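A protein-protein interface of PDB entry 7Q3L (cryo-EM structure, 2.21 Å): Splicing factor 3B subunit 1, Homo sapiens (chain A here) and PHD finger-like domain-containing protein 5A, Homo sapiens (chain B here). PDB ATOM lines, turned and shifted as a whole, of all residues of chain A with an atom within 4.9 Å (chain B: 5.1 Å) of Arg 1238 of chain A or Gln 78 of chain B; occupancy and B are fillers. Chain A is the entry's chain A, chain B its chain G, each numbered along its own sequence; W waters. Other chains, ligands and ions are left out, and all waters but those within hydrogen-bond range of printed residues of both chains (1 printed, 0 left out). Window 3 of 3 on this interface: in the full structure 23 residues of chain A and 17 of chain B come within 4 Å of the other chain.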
ATOM      1  N   LEU A1197      21.337 -27.018   4.378  1.00  0.00           N
ATOM      2  CA  LEU A1197      21.757 -28.369   4.732  1.00  0.00           C
ATOM      3  C   LEU A1197      21.514 -29.382   3.604  1.00  0.00           C
ATOM      4  O   LEU A1197      22.290 -30.322   3.457  1.00  0.00           O
ATOM      5  CB  LEU A1197      21.097 -28.767   6.054  1.00  0.00           C
ATOM      6  CG  LEU A1197      21.543 -27.927   7.251  1.00  0.00           C
ATOM      7  CD1 LEU A1197      20.692 -28.208   8.479  1.00  0.00           C
ATOM      8  CD2 LEU A1197      23.004 -28.176   7.605  1.00  0.00           C
ATOM      9  N   GLY A1232      18.849 -21.310  13.727  1.00  0.00           N
ATOM     10  CA  GLY A1232      18.760 -22.489  12.878  1.00  0.00           C
ATOM     11  C   GLY A1232      19.284 -22.252  11.460  1.00  0.00           C
ATOM     12  O   GLY A1232      20.068 -23.056  10.962  1.00  0.00           O
ATOM     13  N   LEU A1234      21.407 -19.776  10.484  1.00  0.00           N
ATOM     14  CA  LEU A1234      22.839 -19.506  10.573  1.00  0.00           C
ATOM     15  C   LEU A1234      23.660 -20.789  10.757  1.00  0.00           C
ATOM     16  O   LEU A1234      24.680 -20.961  10.101  1.00  0.00           O
ATOM     17  CB  LEU A1234      23.111 -18.486  11.684  1.00  0.00           C
ATOM     18  CG  LEU A1234      22.485 -17.099  11.517  1.00  0.00           C
ATOM     19  CD1 LEU A1234      22.912 -16.194  12.656  1.00  0.00           C
ATOM     20  CD2 LEU A1234      22.849 -16.460  10.183  1.00  0.00           C
ATOM     21  N   GLU A1235      23.196 -21.714  11.606  1.00  0.00           N
ATOM     22  CA  GLU A1235      23.757 -23.052  11.788  1.00  0.00           C
ATOM     23  C   GLU A1235      23.662 -23.915  10.518  1.00  0.00           C
ATOM     24  O   GLU A1235      24.475 -24.817  10.307  1.00  0.00           O
ATOM     25  CB  GLU A1235      23.035 -23.699  12.965  1.00  0.00           C
ATOM     26  CG  GLU A1235      23.835 -23.612  14.243  1.00  0.00           C
ATOM     27  CD  GLU A1235      24.822 -24.760  14.303  1.00  0.00           C
ATOM     28  OE1 GLU A1235      25.996 -24.573  13.900  1.00  0.00           O
ATOM     29  OE2 GLU A1235      24.409 -25.831  14.719  1.00  0.00           O
ATOM     30  N   GLY A1236      22.663 -23.672   9.668  1.00  0.00           N
ATOM     31  CA  GLY A1236      22.589 -24.272   8.345  1.00  0.00           C
ATOM     32  C   GLY A1236      23.634 -23.692   7.386  1.00  0.00           C
ATOM     33  O   GLY A1236      24.348 -24.444   6.726  1.00  0.00           O
ATOM     34  N   LEU A1237      23.730 -22.361   7.317  1.00  0.00           N
ATOM     35  CA  LEU A1237      24.607 -21.655   6.390  1.00  0.00           C
ATOM     36  C   LEU A1237      26.089 -21.802   6.746  1.00  0.00           C
ATOM     37  O   LEU A1237      26.923 -21.808   5.844  1.00  0.00           O
ATOM     38  CB  LEU A1237      24.184 -20.188   6.311  1.00  0.00           C
ATOM     39  CG  LEU A1237      22.796 -19.950   5.723  1.00  0.00           C
ATOM     40  CD1 LEU A1237      22.298 -18.564   6.105  1.00  0.00           C
ATOM     41  CD2 LEU A1237      22.776 -20.094   4.206  1.00  0.00           C
ATOM     42  N   ARG A1238      26.429 -21.982   8.028  1.00  0.00           N
ATOM     43  CA  ARG A1238      27.770 -22.344   8.470  1.00  0.00           C
ATOM     44  C   ARG A1238      28.296 -23.582   7.738  1.00  0.00           C
ATOM     45  O   ARG A1238      29.485 -23.674   7.466  1.00  0.00           O
ATOM     46  CB  ARG A1238      27.790 -22.578   9.981  1.00  0.00           C
ATOM     47  CG  ARG A1238      29.145 -23.024  10.507  1.00  0.00           C
ATOM     48  CD  ARG A1238      29.141 -23.292  11.995  1.00  0.00           C
ATOM     49  NE  ARG A1238      28.274 -24.370  12.425  1.00  0.00           N
ATOM     50  CZ  ARG A1238      28.482 -25.675  12.292  1.00  0.00           C
ATOM     51  NH1 ARG A1238      29.546 -26.153  11.671  1.00  0.00           N
ATOM     52  NH2 ARG A1238      27.582 -26.509  12.782  1.00  0.00           N
ATOM     53  N   VAL A1239      27.412 -24.533   7.440  1.00  0.00           N
ATOM     54  CA  VAL A1239      27.756 -25.751   6.724  1.00  0.00           C
ATOM     55  C   VAL A1239      27.919 -25.486   5.224  1.00  0.00           C
ATOM     56  O   VAL A1239      28.939 -25.849   4.648  1.00  0.00           O
ATOM     57  CB  VAL A1239      26.742 -26.869   7.042  1.00  0.00           C
ATOM     58  CG1 VAL A1239      26.894 -28.072   6.128  1.00  0.00           C
ATOM     59  CG2 VAL A1239      26.864 -27.300   8.492  1.00  0.00           C
ATOM     60  N   ALA A1240      26.938 -24.837   4.584  1.00  0.00           N
ATOM     61  CA  ALA A1240      26.881 -24.725   3.131  1.00  0.00           C
ATOM     62  C   ALA A1240      27.711 -23.577   2.537  1.00  0.00           C
ATOM     63  O   ALA A1240      28.133 -23.681   1.384  1.00  0.00           O
ATOM     64  CB  ALA A1240      25.444 -24.677   2.693  1.00  0.00           C
ATOM     65  N   ILE A1241      27.906 -22.475   3.286  1.00  0.00           N
ATOM     66  CA  ILE A1241      28.784 -21.375   2.896  1.00  0.00           C
ATOM     67  C   ILE A1241      30.148 -21.485   3.590  1.00  0.00           C
ATOM     68  O   ILE A1241      31.154 -20.994   3.077  1.00  0.00           O
ATOM     69  CB  ILE A1241      28.162 -19.984   3.152  1.00  0.00           C
ATOM     70  CG1 ILE A1241      26.706 -19.858   2.696  1.00  0.00           C
ATOM     71  CG2 ILE A1241      29.023 -18.914   2.503  1.00  0.00           C
ATOM     72  CD1 ILE A1241      26.103 -18.496   3.004  1.00  0.00           C
ATOM     73  N   GLY A1242      30.180 -22.122   4.763  1.00  0.00           N
ATOM     74  CA  GLY A1242      31.414 -22.356   5.494  1.00  0.00           C
ATOM     75  C   GLY A1242      31.664 -21.350   6.615  1.00  0.00           C
ATOM     76  O   GLY A1242      31.153 -20.232   6.596  1.00  0.00           O
ATOM     77  N   PRO A1243      32.495 -21.737   7.608  1.00  0.00           N
ATOM     78  CA  PRO A1243      32.782 -20.921   8.786  1.00  0.00           C
ATOM     79  C   PRO A1243      33.499 -19.606   8.502  1.00  0.00           C
ATOM     80  O   PRO A1243      33.339 -18.674   9.273  1.00  0.00           O
ATOM     81  CB  PRO A1243      33.657 -21.834   9.659  1.00  0.00           C
ATOM     82  CG  PRO A1243      34.281 -22.794   8.673  1.00  0.00           C
ATOM     83  CD  PRO A1243      33.186 -23.029   7.657  1.00  0.00           C
ATOM     84  N   MET A1246      30.714 -16.971   7.874  1.00  0.00           N
ATOM     85  CA  MET A1246      30.030 -16.711   9.130  1.00  0.00           C
ATOM     86  C   MET A1246      30.882 -15.864  10.088  1.00  0.00           C
ATOM     87  O   MET A1246      30.353 -14.966  10.749  1.00  0.00           O
ATOM     88  CB  MET A1246      29.625 -18.040   9.763  1.00  0.00           C
ATOM     89  CG  MET A1246      28.747 -18.885   8.853  1.00  0.00           C
ATOM     90  SD  MET A1246      27.218 -18.086   8.293  1.00  0.00           S
ATOM     91  CE  MET A1246      26.342 -17.975   9.851  1.00  0.00           C
ATOM     92  N   SER A1271      28.354 -20.604  18.399  1.00  0.00           N
ATOM     93  CA  SER A1271      27.823 -21.677  17.567  1.00  0.00           C
ATOM     94  C   SER A1271      28.778 -22.015  16.417  1.00  0.00           C
ATOM     95  O   SER A1271      29.059 -23.189  16.181  1.00  0.00           O
ATOM     96  CB  SER A1271      26.409 -21.393  17.105  1.00  0.00           C
ATOM     97  OG  SER A1271      26.381 -20.432  16.058  1.00  0.00           O
ATOM     98  N   ILE A1272      29.338 -20.995  15.751  1.00  0.00           N
ATOM     99  CA  ILE A1272      30.318 -21.179  14.682  1.00  0.00           C
ATOM    100  C   ILE A1272      31.593 -21.837  15.220  1.00  0.00           C
ATOM    101  O   ILE A1272      32.142 -22.742  14.593  1.00  0.00           O
ATOM    102  CB  ILE A1272      30.643 -19.859  13.948  1.00  0.00           C
ATOM    103  CG1 ILE A1272      29.402 -19.163  13.386  1.00  0.00           C
ATOM    104  CG2 ILE A1272      31.680 -20.096  12.854  1.00  0.00           C
ATOM    105  CD1 ILE A1272      29.575 -17.666  13.218  1.00  0.00           C
ATOM    106  N   GLY A1275      30.911 -25.417  16.274  1.00  0.00           N
ATOM    107  CA  GLY A1275      30.703 -26.104  15.008  1.00  0.00           C
ATOM    108  C   GLY A1275      31.977 -26.346  14.192  1.00  0.00           C
ATOM    109  O   GLY A1275      32.077 -27.382  13.548  1.00  0.00           O
ATOM    110  N   SER A1276      32.953 -25.420  14.224  1.00  0.00           N
ATOM    111  CA  SER A1276      34.017 -25.365  13.222  1.00  0.00           C
ATOM    112  C   SER A1276      35.373 -24.895  13.772  1.00  0.00           C
ATOM    113  O   SER A1276      36.142 -24.249  13.049  1.00  0.00           O
ATOM    114  CB  SER A1276      33.594 -24.508  12.047  1.00  0.00           C
ATOM    115  OG  SER A1276      32.427 -25.015  11.417  1.00  0.00           O
ATOM    116  N   GLU B  74      20.139 -34.079   8.863  1.00  0.00           N
ATOM    117  CA  GLU B  74      20.475 -32.690   9.072  1.00  0.00           C
ATOM    118  C   GLU B  74      21.254 -32.554  10.364  1.00  0.00           C
ATOM    119  O   GLU B  74      22.176 -31.806  10.390  1.00  0.00           O
ATOM    120  CB  GLU B  74      19.217 -31.849   9.125  1.00  0.00           C
ATOM    121  CG  GLU B  74      18.647 -31.624   7.750  1.00  0.00           C
ATOM    122  CD  GLU B  74      17.677 -30.463   7.677  1.00  0.00           C
ATOM    123  OE1 GLU B  74      17.386 -29.875   8.739  1.00  0.00           O
ATOM    124  OE2 GLU B  74      17.227 -30.145   6.566  1.00  0.00           O
ATOM    125  N   CYS B  75      20.878 -33.270  11.402  1.00  0.00           N
ATOM    126  CA  CYS B  75      21.592 -33.230  12.655  1.00  0.00           C
ATOM    127  C   CYS B  75      22.963 -33.887  12.558  1.00  0.00           C
ATOM    128  O   CYS B  75      23.823 -33.444  13.233  1.00  0.00           O
ATOM    129  CB  CYS B  75      20.755 -33.846  13.760  1.00  0.00           C
ATOM    130  SG  CYS B  75      19.364 -32.805  14.257  1.00  0.00           S
ATOM    131  N   THR B  76      23.119 -34.953  11.791  1.00  0.00           N
ATOM    132  CA  THR B  76      24.371 -35.672  11.672  1.00  0.00           C
ATOM    133  C   THR B  76      25.363 -34.770  10.971  1.00  0.00           C
ATOM    134  O   THR B  76      26.486 -34.711  11.370  1.00  0.00           O
ATOM    135  CB  THR B  76      24.145 -37.012  10.967  1.00  0.00           C
ATOM    136  OG1 THR B  76      23.350 -37.791  11.857  1.00  0.00           O
ATOM    137  CG2 THR B  76      25.411 -37.734  10.578  1.00  0.00           C
ATOM    138  N   ILE B  77      24.923 -34.042   9.975  1.00  0.00           N
ATOM    139  CA  ILE B  77      25.788 -33.128   9.221  1.00  0.00           C
ATOM    140  C   ILE B  77      26.332 -32.058  10.169  1.00  0.00           C
ATOM    141  O   ILE B  77      27.537 -31.789  10.160  1.00  0.00           O
ATOM    142  CB  ILE B  77      24.994 -32.510   8.051  1.00  0.00           C
ATOM    143  CG1 ILE B  77      24.745 -33.515   6.921  1.00  0.00           C
ATOM    144  CG2 ILE B  77      25.641 -31.223   7.524  1.00  0.00           C
ATOM    145  CD1 ILE B  77      23.700 -33.066   5.928  1.00  0.00           C
ATOM    146  N   GLN B  78      25.451 -31.484  11.004  1.00  0.00           N
ATOM    147  CA  GLN B  78      25.848 -30.414  11.921  1.00  0.00           C
ATOM    148  C   GLN B  78      26.636 -30.963  13.123  1.00  0.00           C
ATOM    149  O   GLN B  78      26.923 -30.184  14.046  1.00  0.00           O
ATOM    150  CB  GLN B  78      24.624 -29.648  12.429  1.00  0.00           C
ATOM    151  CG  GLN B  78      24.324 -28.388  11.636  1.00  0.00           C
ATOM    152  CD  GLN B  78      22.842 -28.136  11.549  1.00  0.00           C
ATOM    153  OE1 GLN B  78      22.026 -29.016  11.813  1.00  0.00           O
ATOM    154  NE2 GLN B  78      22.484 -26.918  11.184  1.00  0.00           N
ATOM    155  N   GLU B  79      26.921 -32.281  13.129  1.00  0.00           N
ATOM    156  CA  GLU B  79      27.695 -32.932  14.204  1.00  0.00           C
ATOM    157  C   GLU B  79      26.932 -32.857  15.527  1.00  0.00           C
ATOM    158  O   GLU B  79      27.560 -32.896  16.582  1.00  0.00           O
ATOM    159  CB  GLU B  79      29.126 -32.399  14.293  1.00  0.00           C
ATOM    160  CG  GLU B  79      29.940 -32.674  13.039  1.00  0.00           C
ATOM    161  CD  GLU B  79      31.423 -32.812  13.312  1.00  0.00           C
ATOM    162  OE1 GLU B  79      31.880 -33.957  13.485  1.00  0.00           O
ATOM    163  OE2 GLU B  79      32.119 -31.776  13.356  1.00  0.00           O
ATOM    164  N   LYS B  80      25.602 -32.741  15.459  1.00  0.00           N
ATOM    165  CA  LYS B  80      24.760 -32.733  16.652  1.00  0.00           C
ATOM    166  C   LYS B  80      24.550 -34.130  17.237  1.00  0.00           C
ATOM    167  O   LYS B  80      24.028 -34.265  18.342  1.00  0.00           O
ATOM    168  CB  LYS B  80      23.447 -32.003  16.377  1.00  0.00           C
ATOM    169  CG  LYS B  80      23.678 -30.518  16.197  1.00  0.00           C
ATOM    170  CD  LYS B  80      22.498 -29.701  15.733  1.00  0.00           C
ATOM    171  CE  LYS B  80      22.947 -28.260  15.660  1.00  0.00           C
ATOM    172  NZ  LYS B  80      22.125 -27.402  14.776  1.00  0.00           N
HETATM  173  O   HOH W   1      20.149 -25.776  12.217  1.00  0.00           O
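The side-chain amide nitrogen of Gln 78 of chain B lies within hydrogen-bond range of the backbone carbonyl oxygen of Glu 1235 of chain A, at 3.0 Å. The side-chain carboxylate (OE2) of Glu 1235 of chain A is in salt-bridge range of the side-chain amino group (NZ) of Lys 80 of chain B.
The backbone carbonyl oxygen of Glu 74 of chain B lies close to the side-chain amide oxygen of Gln 78 of chain B, at 3.1 Å. The backbone NH (N) of Lys 80 of chain B is in hydrogen-bond range of the backbone carbonyl oxygen (O) of Cys 75 of chain B, at 2.9 Å. The side-chain amide oxygen of Gln 78 of chain B is in hydrogen-bond range of the side-chain amino group of Lys 80 of chain B, 3.4 Å away. NE of Arg 1238 of chain A lies within salt-bridge range of OE1 of Glu 1235 of chain A (2.7 Å). The guanidinium group (NH1) of Arg 1238 of chain A sits at hydrogen-bond distance from the backbone carbonyl oxygen (O) of Gly 1275 of chain A (3.4 Å). The guanidinium group of Arg 1238 of chain A is in hydrogen-bond range of the side-chain hydroxyl of Ser 1276 of chain A (3.1 Å).
Among the printed residues, pairs that only touch across the chains: Leu 1197 of chain A with Gln 78 of chain B (3.5 Å), Gly 1236 of chain A with Gln 78 of chain B (3.6 Å), Val 1239 of chain A with Ile 77 of chain B (3.7 Å), Leu 1197 of chain A with Glu 74 of chain B (3.7 Å), Arg 1238 of chain A with Gln 78 of chain B (3.9 Å) and Leu 1197 of chain A with Ile 77 of chain B (3.95 Å).
Printed residues of chain B within 4 Å of Val 1239 of chain A: Ile 77. Printed residues of chain A within 4 Å of Glu 74 of chain B: Leu 1197. Printed residues of chain A within 4 Å of Ile 77 of chain B: Leu 1197 (3.95 Å) and Val 1239 (3.7 Å). Of chain A, only Leu 1197 (3.5 Å), Glu 1235 (3.0 Å), Gly 1236 (3.6 Å) and Arg 1238 (3.9 Å) come within 4 Å of Gln 78 of chain B. Of the printed residues of chain A, Lys 80 of chain B touches Glu 1235 (2.8 Å). The nearest residue of chain A that does not touch Gln 78 of chain B is Val 1239 of chain A (4.2 Å). The nearest printed residue of chain A that does not touch Glu 74 of chain B is Val 1239 of chain A (6.8 Å).
Of the 17 printed residues of chain A, 5 touch a printed residue of chain B. Of the 7 printed residues of chain B, 4 touch a printed residue of chain A. Hydrophobic or aromatic side chains of chain B within 4 Å of the printed part of chain A: Ile 77. Among the printed residues, 8 pairs touch across the chains. Among the printed residues, Asp or Glu carboxylates within 4 Å of a Lys or Arg side-chain nitrogen of the other chain: Glu 1235 of chain A with Lys 80 of chain B.
Water W1 bridges NE2 of Gln 78 of chain B and O of Gly 1232 of chain A.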
